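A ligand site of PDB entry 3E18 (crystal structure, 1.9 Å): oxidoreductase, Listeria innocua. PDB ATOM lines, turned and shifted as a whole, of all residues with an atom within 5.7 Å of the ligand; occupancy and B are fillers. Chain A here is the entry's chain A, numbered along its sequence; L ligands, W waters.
Water W3 bridges O1 of the ligand (2.8 Å) and NZ of Lys 42 (3.2 Å). Water W6 lies within hydrogen-bond range of O of Ala 72, O9 of the ligand, N of Gly 17, N of Gly 14 and O of Gly 12. Water W7 lies within hydrogen-bond range of the side-chain amide nitrogen of Asn 75 (2.9 Å), an oxygen (O13) of the ligand (3.2 Å) and the backbone carbonyl oxygen of Leu 175 (3.3 Å).
N of Glu 95 lies within hydrogen-bond range of O of Ile 71, 3.0 Å away. ND1 of His 78 sits close to O of Glu 95, at 3.5 Å. A ring nitrogen (ND1) of His 78 lies within hydrogen-bond range of the backbone carbonyl oxygen (O) of Pro 97 (3.0 Å). NH1 of Arg 164 is in salt-bridge range of OD1 of Asp 162, 3.7 Å away. O of Val 11 is in hydrogen-bond range of N of Ala 72, at 2.8 Å. The side-chain amide oxygen (OD1) of Asn 124 sits close to the backbone carbonyl oxygen (O) of His 122, at 3.5 Å. O of Pro 74 sits at hydrogen-bond distance from OG of Ser 77. OE2 of Glu 95 lies within hydrogen-bond range of ND1 of His 122 (2.8 Å).
Merely in contact with the ligand: Val 11 (3.97 Å), Gly 12 (3.5 Å), Tyr 13 (3.8 Å), Gly 14 (3.2 Å), Phe 36 (3.7 Å), Leu 39 (3.7 Å), Ala 72 (3.3 Å), Pro 74 (3.5 Å), Pro 97 (3.8 Å), His 122 (3.97 Å) and Asp 162 (3.9 Å). Hydrophobic or aromatic side chains within 4 Å of the ligand: Val 11, Met 16, Phe 36, Ile 38, Leu 39, Pro 74, His 78, Pro 97, Trp 163 and His 180.
The backbone carbonyl oxygen of Lys 96 sits at hydrogen-bond distance from an oxygen (O13) of the ligand (2.6 Å). The backbone NH (N) of Met 16 is in hydrogen-bond range of an oxygen (O9) of the ligand (2.8 Å). A nitrogen (N7) of the ligand is in hydrogen-bond range of the side-chain carboxylate of Glu 95, 2.9 Å away. An oxygen (O12) of the ligand lies within hydrogen-bond range of the side-chain amide oxygen (OD1) of Asn 75 (2.7 Å). NZ of Lys 42 is in hydrogen-bond range of O5 of the ligand, 2.7 Å away. An oxygen (O12) of the ligand sits at hydrogen-bond distance from the backbone carbonyl oxygen (O) of Thr 73, 3.3 Å away. NZ of Lys 96 sits at hydrogen-bond distance from O13 of the ligand, 3.2 Å away. The backbone NH of Gly 15 is in hydrogen-bond range of an oxygen (O1) of the ligand, 3.1 Å away. The guanidinium group of Arg 164 lies within salt-bridge range of an oxygen (O8) of the ligand, at 2.7 Å. The side-chain amide oxygen (OD1) of Asn 124 lies within hydrogen-bond range of a nitrogen (N7) of the ligand (3.0 Å). The side-chain carboxylate (OD1) of Asp 37 sits at hydrogen-bond distance from an oxygen (O6) of the ligand, 2.8 Å away. NE2 of His 78 sits close to O12 of the ligand, 3.1 Å away. O14 of the ligand lies within hydrogen-bond range of NE2 of His 180, 3.5 Å away. NE1 of Trp 163 sits at hydrogen-bond distance from O2 of the ligand, 2.9 Å away. N5 of the ligand lies within hydrogen-bond range of N of Ile 38, at 3.4 Å.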
ATOM      1  N   VAL A  11     -12.202 -20.664  13.077  1.00  0.00           N
ATOM      2  CA  VAL A  11     -12.652 -19.838  14.199  1.00  0.00           C
ATOM      3  C   VAL A  11     -13.704 -20.619  14.989  1.00  0.00           C
ATOM      4  O   VAL A  11     -14.845 -20.798  14.556  1.00  0.00           O
ATOM      5  CB  VAL A  11     -13.265 -18.494  13.729  1.00  0.00           C
ATOM      6  CG1 VAL A  11     -13.617 -17.623  14.906  1.00  0.00           C
ATOM      7  CG2 VAL A  11     -12.293 -17.768  12.798  1.00  0.00           C
ATOM      8  N   GLY A  12     -13.306 -21.073  16.178  1.00  0.00           N
ATOM      9  CA  GLY A  12     -14.153 -21.952  16.960  1.00  0.00           C
ATOM     10  C   GLY A  12     -13.577 -23.348  16.870  1.00  0.00           C
ATOM     11  O   GLY A  12     -13.912 -24.109  15.977  1.00  0.00           O
ATOM     12  N   TYR A  13     -12.689 -23.680  17.804  1.00  0.00           N
ATOM     13  CA  TYR A  13     -12.039 -24.981  17.784  1.00  0.00           C
ATOM     14  C   TYR A  13     -12.747 -25.963  18.717  1.00  0.00           C
ATOM     15  O   TYR A  13     -12.168 -26.496  19.673  1.00  0.00           O
ATOM     16  CB  TYR A  13     -10.557 -24.844  18.101  1.00  0.00           C
ATOM     17  CG  TYR A  13      -9.746 -26.072  17.768  1.00  0.00           C
ATOM     18  CD1 TYR A  13      -9.497 -26.415  16.442  1.00  0.00           C
ATOM     19  CD2 TYR A  13      -9.230 -26.891  18.773  1.00  0.00           C
ATOM     20  CE1 TYR A  13      -8.750 -27.555  16.125  1.00  0.00           C
ATOM     21  CE2 TYR A  13      -8.499 -28.021  18.477  1.00  0.00           C
ATOM     22  CZ  TYR A  13      -8.255 -28.343  17.156  1.00  0.00           C
ATOM     23  OH  TYR A  13      -7.518 -29.471  16.873  1.00  0.00           O
ATOM     24  N   GLY A  14     -14.021 -26.224  18.444  1.00  0.00           N
ATOM     25  CA  GLY A  14     -14.785 -27.175  19.236  1.00  0.00           C
ATOM     26  C   GLY A  14     -14.930 -28.465  18.475  1.00  0.00           C
ATOM     27  O   GLY A  14     -14.082 -28.802  17.659  1.00  0.00           O
ATOM     28  N   GLY A  15     -16.035 -29.173  18.723  1.00  0.00           N
ATOM     29  CA  GLY A  15     -16.311 -30.439  18.048  1.00  0.00           C
ATOM     30  C   GLY A  15     -16.237 -30.380  16.526  1.00  0.00           C
ATOM     31  O   GLY A  15     -15.482 -31.142  15.910  1.00  0.00           O
ATOM     32  N   MET A  16     -17.000 -29.474  15.926  1.00  0.00           N
ATOM     33  CA  MET A  16     -17.055 -29.382  14.480  1.00  0.00           C
ATOM     34  C   MET A  16     -15.860 -28.617  13.890  1.00  0.00           C
ATOM     35  O   MET A  16     -15.353 -28.972  12.822  1.00  0.00           O
ATOM     36  CB  MET A  16     -18.367 -28.720  14.047  1.00  0.00           C
ATOM     37  CG  MET A  16     -18.750 -28.968  12.594  1.00  0.00           C
ATOM     38  SD  MET A  16     -18.820 -30.717  12.089  1.00  0.00           S
ATOM     39  CE  MET A  16     -19.051 -30.527  10.334  1.00  0.00           C
ATOM     40  N   GLY A  17     -15.434 -27.571  14.586  1.00  0.00           N
ATOM     41  CA  GLY A  17     -14.282 -26.772  14.184  1.00  0.00           C
ATOM     42  C   GLY A  17     -13.020 -27.600  14.057  1.00  0.00           C
ATOM     43  O   GLY A  17     -12.286 -27.454  13.085  1.00  0.00           O
ATOM     44  N   PHE A  36      -8.240 -19.919  15.601  1.00  0.00           N
ATOM     45  CA  PHE A  36      -8.567 -19.099  16.763  1.00  0.00           C
ATOM     46  C   PHE A  36      -9.733 -19.682  17.560  1.00  0.00           C
ATOM     47  O   PHE A  36     -10.722 -20.141  16.978  1.00  0.00           O
ATOM     48  CB  PHE A  36      -8.890 -17.644  16.372  1.00  0.00           C
ATOM     49  CG  PHE A  36      -9.323 -16.801  17.537  1.00  0.00           C
ATOM     50  CD1 PHE A  36      -8.412 -16.452  18.531  1.00  0.00           C
ATOM     51  CD2 PHE A  36     -10.646 -16.406  17.675  1.00  0.00           C
ATOM     52  CE1 PHE A  36      -8.807 -15.709  19.647  1.00  0.00           C
ATOM     53  CE2 PHE A  36     -11.052 -15.654  18.778  1.00  0.00           C
ATOM     54  CZ  PHE A  36     -10.124 -15.306  19.756  1.00  0.00           C
ATOM     55  N   ASP A  37      -9.603 -19.655  18.879  1.00  0.00           N
ATOM     56  CA  ASP A  37     -10.717 -19.927  19.777  1.00  0.00           C
ATOM     57  C   ASP A  37     -10.670 -18.911  20.903  1.00  0.00           C
ATOM     58  O   ASP A  37      -9.605 -18.428  21.269  1.00  0.00           O
ATOM     59  CB  ASP A  37     -10.668 -21.363  20.300  1.00  0.00           C
ATOM     60  CG  ASP A  37     -12.005 -21.820  20.882  1.00  0.00           C
ATOM     61  OD1 ASP A  37     -12.387 -21.341  21.982  1.00  0.00           O
ATOM     62  OD2 ASP A  37     -12.665 -22.686  20.268  1.00  0.00           O
ATOM     63  N   ILE A  38     -11.840 -18.575  21.446  1.00  0.00           N
ATOM     64  CA  ILE A  38     -11.925 -17.608  22.541  1.00  0.00           C
ATOM     65  C   ILE A  38     -11.349 -18.159  23.869  1.00  0.00           C
ATOM     66  O   ILE A  38     -10.854 -17.401  24.697  1.00  0.00           O
ATOM     67  CB  ILE A  38     -13.366 -17.048  22.694  1.00  0.00           C
ATOM     68  CG1 ILE A  38     -13.356 -15.708  23.426  1.00  0.00           C
ATOM     69  CG2 ILE A  38     -14.304 -18.086  23.308  1.00  0.00           C
ATOM     70  CD1 ILE A  38     -14.618 -14.885  23.244  1.00  0.00           C
ATOM     71  N   LEU A  39     -11.388 -19.477  24.038  1.00  0.00           N
ATOM     72  CA  LEU A  39     -10.809 -20.109  25.225  1.00  0.00           C
ATOM     73  C   LEU A  39      -9.347 -20.471  24.991  1.00  0.00           C
ATOM     74  O   LEU A  39      -8.994 -21.051  23.960  1.00  0.00           O
ATOM     75  CB  LEU A  39     -11.612 -21.344  25.632  1.00  0.00           C
ATOM     76  CG  LEU A  39     -13.085 -21.196  26.016  1.00  0.00           C
ATOM     77  CD1 LEU A  39     -13.665 -22.545  26.370  1.00  0.00           C
ATOM     78  CD2 LEU A  39     -13.302 -20.222  27.186  1.00  0.00           C
ATOM     79  N   LYS A  42      -8.740 -24.209  24.449  1.00  0.00           N
ATOM     80  CA  LYS A  42      -8.930 -24.702  23.099  1.00  0.00           C
ATOM     81  C   LYS A  42      -7.831 -24.261  22.144  1.00  0.00           C
ATOM     82  O   LYS A  42      -7.538 -24.965  21.178  1.00  0.00           O
ATOM     83  CB  LYS A  42     -10.324 -24.339  22.584  1.00  0.00           C
ATOM     84  CG  LYS A  42     -11.266 -25.541  22.569  1.00  0.00           C
ATOM     85  CD  LYS A  42     -11.743 -25.963  23.933  1.00  0.00           C
ATOM     86  CE  LYS A  42     -13.177 -25.519  24.190  1.00  0.00           C
ATOM     87  NZ  LYS A  42     -14.179 -26.157  23.282  1.00  0.00           N
ATOM     88  N   ILE A  71     -16.306 -20.335  10.295  1.00  0.00           N
ATOM     89  CA  ILE A  71     -16.953 -20.047  11.587  1.00  0.00           C
ATOM     90  C   ILE A  71     -17.681 -21.252  12.151  1.00  0.00           C
ATOM     91  O   ILE A  71     -18.705 -21.685  11.635  1.00  0.00           O
ATOM     92  CB  ILE A  71     -17.883 -18.801  11.502  1.00  0.00           C
ATOM     93  CG1 ILE A  71     -17.032 -17.574  11.154  1.00  0.00           C
ATOM     94  CG2 ILE A  71     -18.624 -18.529  12.832  1.00  0.00           C
ATOM     95  CD1 ILE A  71     -17.800 -16.520  10.457  1.00  0.00           C
ATOM     96  N   ALA A  72     -17.121 -21.811  13.226  1.00  0.00           N
ATOM     97  CA  ALA A  72     -17.724 -22.959  13.879  1.00  0.00           C
ATOM     98  C   ALA A  72     -17.921 -22.695  15.373  1.00  0.00           C
ATOM     99  O   ALA A  72     -17.557 -23.515  16.234  1.00  0.00           O
ATOM    100  CB  ALA A  72     -16.885 -24.203  13.630  1.00  0.00           C
ATOM    101  N   THR A  73     -18.498 -21.538  15.680  1.00  0.00           N
ATOM    102  CA  THR A  73     -18.811 -21.128  17.051  1.00  0.00           C
ATOM    103  C   THR A  73     -20.309 -21.396  17.305  1.00  0.00           C
ATOM    104  O   THR A  73     -21.028 -21.707  16.357  1.00  0.00           O
ATOM    105  CB  THR A  73     -18.498 -19.633  17.240  1.00  0.00           C
ATOM    106  OG1 THR A  73     -19.333 -18.868  16.364  1.00  0.00           O
ATOM    107  CG2 THR A  73     -17.041 -19.346  16.944  1.00  0.00           C
ATOM    108  N   PRO A  74     -20.777 -21.309  18.577  1.00  0.00           N
ATOM    109  CA  PRO A  74     -22.228 -21.373  18.826  1.00  0.00           C
ATOM    110  C   PRO A  74     -23.049 -20.369  17.998  1.00  0.00           C
ATOM    111  O   PRO A  74     -22.530 -19.342  17.541  1.00  0.00           O
ATOM    112  CB  PRO A  74     -22.344 -21.097  20.320  1.00  0.00           C
ATOM    113  CG  PRO A  74     -21.054 -21.618  20.881  1.00  0.00           C
ATOM    114  CD  PRO A  74     -20.018 -21.245  19.852  1.00  0.00           C
ATOM    115  N   ASN A  75     -24.324 -20.666  17.806  1.00  0.00           N
ATOM    116  CA  ASN A  75     -25.129 -19.994  16.786  1.00  0.00           C
ATOM    117  C   ASN A  75     -25.311 -18.490  16.923  1.00  0.00           C
ATOM    118  O   ASN A  75     -25.467 -17.786  15.914  1.00  0.00           O
ATOM    119  CB  ASN A  75     -26.497 -20.658  16.683  1.00  0.00           C
ATOM    120  CG  ASN A  75     -26.408 -22.077  16.202  1.00  0.00           C
ATOM    121  OD1 ASN A  75     -25.435 -22.464  15.531  1.00  0.00           O
ATOM    122  ND2 ASN A  75     -27.420 -22.881  16.525  1.00  0.00           N
ATOM    123  N   SER A  77     -23.206 -16.241  17.866  1.00  0.00           N
ATOM    124  CA  SER A  77     -22.042 -15.452  17.477  1.00  0.00           C
ATOM    125  C   SER A  77     -21.743 -15.427  15.962  1.00  0.00           C
ATOM    126  O   SER A  77     -20.850 -14.716  15.533  1.00  0.00           O
ATOM    127  CB  SER A  77     -20.797 -15.907  18.266  1.00  0.00           C
ATOM    128  OG  SER A  77     -20.580 -17.304  18.119  1.00  0.00           O
ATOM    129  N   HIS A  78     -22.501 -16.188  15.161  1.00  0.00           N
ATOM    130  CA  HIS A  78     -22.162 -16.357  13.753  1.00  0.00           C
ATOM    131  C   HIS A  78     -22.196 -15.048  12.967  1.00  0.00           C
ATOM    132  O   HIS A  78     -21.314 -14.785  12.171  1.00  0.00           O
ATOM    133  CB  HIS A  78     -23.115 -17.321  13.043  1.00  0.00           C
ATOM    134  CG  HIS A  78     -22.942 -18.763  13.436  1.00  0.00           C
ATOM    135  ND1 HIS A  78     -23.763 -19.747  12.948  1.00  0.00           N
ATOM    136  CD2 HIS A  78     -22.057 -19.371  14.253  1.00  0.00           C
ATOM    137  CE1 HIS A  78     -23.393 -20.916  13.458  1.00  0.00           C
ATOM    138  NE2 HIS A  78     -22.364 -20.709  14.255  1.00  0.00           N
ATOM    139  N   LEU A  81     -19.212 -12.352  13.765  1.00  0.00           N
ATOM    140  CA  LEU A  81     -17.941 -12.875  13.267  1.00  0.00           C
ATOM    141  C   LEU A  81     -17.878 -12.905  11.748  1.00  0.00           C
ATOM    142  O   LEU A  81     -16.835 -12.613  11.172  1.00  0.00           O
ATOM    143  CB  LEU A  81     -17.650 -14.260  13.848  1.00  0.00           C
ATOM    144  CG  LEU A  81     -17.621 -14.352  15.378  1.00  0.00           C
ATOM    145  CD1 LEU A  81     -17.424 -15.796  15.857  1.00  0.00           C
ATOM    146  CD2 LEU A  81     -16.575 -13.444  15.996  1.00  0.00           C
ATOM    147  N   GLU A  95     -20.830 -22.412   9.627  1.00  0.00           N
ATOM    148  CA  GLU A  95     -21.635 -23.540  10.042  1.00  0.00           C
ATOM    149  C   GLU A  95     -23.134 -23.260  10.152  1.00  0.00           C
ATOM    150  O   GLU A  95     -23.557 -22.139  10.403  1.00  0.00           O
ATOM    151  CB  GLU A  95     -21.123 -24.096  11.361  1.00  0.00           C
ATOM    152  CG  GLU A  95     -20.113 -25.210  11.187  1.00  0.00           C
ATOM    153  CD  GLU A  95     -20.673 -26.431  10.426  1.00  0.00           C
ATOM    154  OE1 GLU A  95     -21.889 -26.514  10.148  1.00  0.00           O
ATOM    155  OE2 GLU A  95     -19.869 -27.308  10.077  1.00  0.00           O
ATOM    156  N   LYS A  96     -23.919 -24.311   9.918  1.00  0.00           N
ATOM    157  CA  LYS A  96     -25.380 -24.313  10.085  1.00  0.00           C
ATOM    158  C   LYS A  96     -25.757 -24.188  11.568  1.00  0.00           C
ATOM    159  O   LYS A  96     -24.988 -24.611  12.443  1.00  0.00           O
ATOM    160  CB  LYS A  96     -25.982 -25.607   9.504  1.00  0.00           C
ATOM    161  CG  LYS A  96     -25.492 -26.919  10.167  1.00  0.00           C
ATOM    162  CD  LYS A  96     -26.603 -27.632  10.968  1.00  0.00           C
ATOM    163  CE  LYS A  96     -26.610 -27.349  12.466  1.00  0.00           C
ATOM    164  NZ  LYS A  96     -25.889 -28.349  13.292  1.00  0.00           N
ATOM    165  N   PRO A  97     -26.921 -23.572  11.891  1.00  0.00           N
ATOM    166  CA  PRO A  97     -27.766 -22.686  11.086  1.00  0.00           C
ATOM    167  C   PRO A  97     -26.935 -21.412  10.976  1.00  0.00           C
ATOM    168  O   PRO A  97     -26.227 -21.059  11.935  1.00  0.00           O
ATOM    169  CB  PRO A  97     -29.013 -22.485  11.958  1.00  0.00           C
ATOM    170  CG  PRO A  97     -28.574 -22.738  13.344  1.00  0.00           C
ATOM    171  CD  PRO A  97     -27.470 -23.771  13.243  1.00  0.00           C
ATOM    172  N   HIS A 122     -22.299 -24.075   5.375  1.00  0.00           N
ATOM    173  CA  HIS A 122     -21.857 -25.449   5.342  1.00  0.00           C
ATOM    174  C   HIS A 122     -23.026 -26.412   5.464  1.00  0.00           C
ATOM    175  O   HIS A 122     -23.251 -27.007   6.521  1.00  0.00           O
ATOM    176  CB  HIS A 122     -20.852 -25.716   6.469  1.00  0.00           C
ATOM    177  CG  HIS A 122     -20.140 -27.019   6.318  1.00  0.00           C
ATOM    178  ND1 HIS A 122     -19.931 -27.874   7.378  1.00  0.00           N
ATOM    179  CD2 HIS A 122     -19.603 -27.622   5.231  1.00  0.00           C
ATOM    180  CE1 HIS A 122     -19.283 -28.944   6.955  1.00  0.00           C
ATOM    181  NE2 HIS A 122     -19.060 -28.821   5.660  1.00  0.00           N
ATOM    182  N   ASN A 124     -23.496 -29.525   4.732  1.00  0.00           N
ATOM    183  CA  ASN A 124     -22.787 -30.736   4.361  1.00  0.00           C
ATOM    184  C   ASN A 124     -23.702 -31.942   4.152  1.00  0.00           C
ATOM    185  O   ASN A 124     -23.332 -32.887   3.454  1.00  0.00           O
ATOM    186  CB  ASN A 124     -21.719 -31.087   5.431  1.00  0.00           C
ATOM    187  CG  ASN A 124     -22.309 -31.225   6.820  1.00  0.00           C
ATOM    188  OD1 ASN A 124     -23.129 -30.413   7.225  1.00  0.00           O
ATOM    189  ND2 ASN A 124     -21.881 -32.237   7.569  1.00  0.00           N
ATOM    190  N   ARG A 125     -24.900 -31.924   4.718  1.00  0.00           N
ATOM    191  CA  ARG A 125     -25.783 -33.097   4.614  1.00  0.00           C
ATOM    192  C   ARG A 125     -26.534 -33.213   3.292  1.00  0.00           C
ATOM    193  O   ARG A 125     -27.245 -34.194   3.047  1.00  0.00           O
ATOM    194  CB  ARG A 125     -26.675 -33.239   5.849  1.00  0.00           C
ATOM    195  CG  ARG A 125     -25.832 -33.579   7.092  1.00  0.00           C
ATOM    196  CD  ARG A 125     -26.645 -34.231   8.187  1.00  0.00           C
ATOM    197  NE  ARG A 125     -25.795 -34.673   9.300  1.00  0.00           N
ATOM    198  CZ  ARG A 125     -25.313 -35.907   9.462  1.00  0.00           C
ATOM    199  NH1 ARG A 125     -25.584 -36.879   8.597  1.00  0.00           N
ATOM    200  NH2 ARG A 125     -24.578 -36.170  10.522  1.00  0.00           N
ATOM    201  N   ASP A 162     -24.739 -28.840  26.944  1.00  0.00           N
ATOM    202  CA  ASP A 162     -23.953 -27.644  26.523  1.00  0.00           C
ATOM    203  C   ASP A 162     -24.852 -26.492  26.031  1.00  0.00           C
ATOM    204  O   ASP A 162     -26.044 -26.449  26.366  1.00  0.00           O
ATOM    205  CB  ASP A 162     -22.664 -27.887  25.673  1.00  0.00           C
ATOM    206  CG  ASP A 162     -22.918 -28.045  24.146  1.00  0.00           C
ATOM    207  OD1 ASP A 162     -24.063 -27.876  23.632  1.00  0.00           O
ATOM    208  OD2 ASP A 162     -21.925 -28.355  23.457  1.00  0.00           O
ATOM    209  N   TRP A 163     -24.296 -25.560  25.268  1.00  0.00           N
ATOM    210  CA  TRP A 163     -24.996 -24.370  24.771  1.00  0.00           C
ATOM    211  C   TRP A 163     -26.259 -24.647  23.939  1.00  0.00           C
ATOM    212  O   TRP A 163     -27.107 -23.769  23.775  1.00  0.00           O
ATOM    213  CB  TRP A 163     -24.024 -23.493  23.971  1.00  0.00           C
ATOM    214  CG  TRP A 163     -23.428 -24.176  22.757  1.00  0.00           C
ATOM    215  CD1 TRP A 163     -22.243 -24.858  22.687  1.00  0.00           C
ATOM    216  CD2 TRP A 163     -24.008 -24.234  21.437  1.00  0.00           C
ATOM    217  NE1 TRP A 163     -22.051 -25.332  21.402  1.00  0.00           N
ATOM    218  CE2 TRP A 163     -23.121 -24.963  20.624  1.00  0.00           C
ATOM    219  CE3 TRP A 163     -25.192 -23.730  20.879  1.00  0.00           C
ATOM    220  CZ2 TRP A 163     -23.366 -25.203  19.272  1.00  0.00           C
ATOM    221  CZ3 TRP A 163     -25.445 -23.972  19.531  1.00  0.00           C
ATOM    222  CH2 TRP A 163     -24.541 -24.709  18.744  1.00  0.00           C
ATOM    223  N   ARG A 164     -26.352 -25.861  23.390  1.00  0.00           N
ATOM    224  CA  ARG A 164     -27.538 -26.325  22.670  1.00  0.00           C
ATOM    225  C   ARG A 164     -28.802 -26.479  23.515  1.00  0.00           C
ATOM    226  O   ARG A 164     -29.896 -26.635  22.966  1.00  0.00           O
ATOM    227  CB  ARG A 164     -27.229 -27.649  21.978  1.00  0.00           C
ATOM    228  CG  ARG A 164     -26.549 -27.502  20.625  1.00  0.00           C
ATOM    229  CD  ARG A 164     -26.334 -28.872  19.994  1.00  0.00           C
ATOM    230  NE  ARG A 164     -25.411 -28.836  18.865  1.00  0.00           N
ATOM    231  CZ  ARG A 164     -24.088 -28.883  18.981  1.00  0.00           C
ATOM    232  NH1 ARG A 164     -23.506 -28.952  20.170  1.00  0.00           N
ATOM    233  NH2 ARG A 164     -23.337 -28.849  17.892  1.00  0.00           N
ATOM    234  N   LEU A 175     -33.201 -26.064  15.240  1.00  0.00           N
ATOM    235  CA  LEU A 175     -32.005 -25.363  14.801  1.00  0.00           C
ATOM    236  C   LEU A 175     -30.787 -26.282  14.596  1.00  0.00           C
ATOM    237  O   LEU A 175     -29.850 -25.947  13.884  1.00  0.00           O
ATOM    238  CB  LEU A 175     -31.701 -24.219  15.785  1.00  0.00           C
ATOM    239  CG  LEU A 175     -32.693 -23.055  15.660  1.00  0.00           C
ATOM    240  CD1 LEU A 175     -32.485 -22.025  16.780  1.00  0.00           C
ATOM    241  CD2 LEU A 175     -32.565 -22.404  14.317  1.00  0.00           C
ATOM    242  N   ASP A 176     -30.820 -27.458  15.206  1.00  0.00           N
ATOM    243  CA  ASP A 176     -29.713 -28.389  15.119  1.00  0.00           C
ATOM    244  C   ASP A 176     -29.888 -29.346  13.935  1.00  0.00           C
ATOM    245  O   ASP A 176     -29.179 -29.258  12.941  1.00  0.00           O
ATOM    246  CB  ASP A 176     -29.592 -29.157  16.431  1.00  0.00           C
ATOM    247  CG  ASP A 176     -28.318 -29.963  16.540  1.00  0.00           C
ATOM    248  OD1 ASP A 176     -27.505 -29.975  15.593  1.00  0.00           O
ATOM    249  OD2 ASP A 176     -28.124 -30.611  17.591  1.00  0.00           O
ATOM    250  N   HIS A 180     -30.731 -29.161   8.753  1.00  0.00           N
ATOM    251  CA  HIS A 180     -30.255 -30.156   7.771  1.00  0.00           C
ATOM    252  C   HIS A 180     -31.399 -30.774   6.971  1.00  0.00           C
ATOM    253  O   HIS A 180     -31.308 -30.888   5.745  1.00  0.00           O
ATOM    254  CB  HIS A 180     -29.565 -31.312   8.471  1.00  0.00           C
ATOM    255  CG  HIS A 180     -28.193 -31.009   8.952  1.00  0.00           C
ATOM    256  ND1 HIS A 180     -27.254 -30.376   8.177  1.00  0.00           N
ATOM    257  CD2 HIS A 180     -27.586 -31.314  10.121  1.00  0.00           C
ATOM    258  CE1 HIS A 180     -26.122 -30.291   8.852  1.00  0.00           C
ATOM    259  NE2 HIS A 180     -26.295 -30.843  10.034  1.00  0.00           N
HETATM  260  P1  LIG L   1     -18.678 -26.596  20.496  1.00  0.00           P
HETATM  261  O1  LIG L   1     -18.171 -27.985  20.548  1.00  0.00           O
HETATM  262  O2  LIG L   1     -19.248 -26.115  21.763  1.00  0.00           O
HETATM  263  O3  LIG L   1     -17.517 -25.612  19.983  1.00  0.00           O
HETATM  264  C1  LIG L   1     -17.709 -24.225  19.777  1.00  0.00           C
HETATM  265  C2  LIG L   1     -16.356 -23.555  19.989  1.00  0.00           C
HETATM  266  O4  LIG L   1     -16.425 -22.181  19.667  1.00  0.00           O
HETATM  267  C3  LIG L   1     -15.915 -23.659  21.443  1.00  0.00           C
HETATM  268  O5  LIG L   1     -14.614 -24.210  21.480  1.00  0.00           O
HETATM  269  C4  LIG L   1     -15.909 -22.223  21.932  1.00  0.00           C
HETATM  270  O6  LIG L   1     -14.910 -21.968  22.883  1.00  0.00           O
HETATM  271  C5  LIG L   1     -15.702 -21.444  20.649  1.00  0.00           C
HETATM  272  N1  LIG L   1     -16.218 -20.062  20.707  1.00  0.00           N
HETATM  273  C6  LIG L   1     -17.353 -19.614  21.350  1.00  0.00           C
HETATM  274  N2  LIG L   1     -17.458 -18.290  21.144  1.00  0.00           N
HETATM  275  C7  LIG L   1     -16.411 -17.880  20.379  1.00  0.00           C
HETATM  276  C8  LIG L   1     -16.035 -16.645  19.883  1.00  0.00           C
HETATM  277  N3  LIG L   1     -16.866 -15.603  20.000  1.00  0.00           N
HETATM  278  N4  LIG L   1     -14.880 -16.535  19.116  1.00  0.00           N
HETATM  279  C9  LIG L   1     -14.115 -17.650  18.848  1.00  0.00           C
HETATM  280  N5  LIG L   1     -14.498 -18.879  19.338  1.00  0.00           N
HETATM  281  C10 LIG L   1     -15.630 -18.996  20.097  1.00  0.00           C
HETATM  282  O7  LIG L   1     -19.798 -26.494  19.326  1.00  0.00           O
HETATM  283  P2  LIG L   1     -19.875 -27.451  18.057  1.00  0.00           P
HETATM  284  O8  LIG L   1     -20.724 -28.632  18.377  1.00  0.00           O
HETATM  285  O9  LIG L   1     -18.543 -27.644  17.453  1.00  0.00           O
HETATM  286  O10 LIG L   1     -20.775 -26.542  17.041  1.00  0.00           O
HETATM  287  C11 LIG L   1     -20.362 -25.268  16.574  1.00  0.00           C
HETATM  288  C12 LIG L   1     -21.156 -24.900  15.310  1.00  0.00           C
HETATM  289  O11 LIG L   1     -21.096 -25.956  14.367  1.00  0.00           O
HETATM  290  C13 LIG L   1     -22.637 -24.669  15.567  1.00  0.00           C
HETATM  291  O12 LIG L   1     -23.121 -23.670  14.687  1.00  0.00           O
HETATM  292  C14 LIG L   1     -23.306 -25.976  15.203  1.00  0.00           C
HETATM  293  O13 LIG L   1     -24.606 -25.740  14.722  1.00  0.00           O
HETATM  294  C15 LIG L   1     -22.392 -26.474  14.085  1.00  0.00           C
HETATM  295  N6  LIG L   1     -22.365 -27.954  13.886  1.00  0.00           N
HETATM  296  C16 LIG L   1     -22.657 -28.410  12.638  1.00  0.00           C
HETATM  297  C17 LIG L   1     -22.657 -29.767  12.327  1.00  0.00           C
HETATM  298  C18 LIG L   1     -22.745 -30.174  10.894  1.00  0.00           C
HETATM  299  O14 LIG L   1     -22.953 -31.528  10.583  1.00  0.00           O
HETATM  300  N7  LIG L   1     -22.631 -29.269   9.928  1.00  0.00           N
HETATM  301  C19 LIG L   1     -22.310 -30.690  13.324  1.00  0.00           C
HETATM  302  C20 LIG L   1     -21.991 -30.222  14.604  1.00  0.00           C
HETATM  303  C21 LIG L   1     -22.020 -28.847  14.876  1.00  0.00           C
HETATM  304  O   HOH W   1     -16.460 -20.702  24.857  1.00  0.00           O
HETATM  305  O   HOH W   2     -13.505 -13.570  19.575  1.00  0.00           O
HETATM  306  O   HOH W   3     -16.014 -28.516  22.263  1.00  0.00           O
HETATM  307  O   HOH W   4     -20.064 -17.215  23.046  1.00  0.00           O
HETATM  308  O   HOH W   5     -19.153 -30.686  21.223  1.00  0.00           O
HETATM  309  O   HOH W   6     -16.400 -25.956  16.750  1.00  0.00           O
HETATM  310  O   HOH W   7     -27.481 -25.743  16.165  1.00  0.00           O
HETATM  311  O   HOH W   8     -19.056 -14.858  21.930  1.00  0.00           O
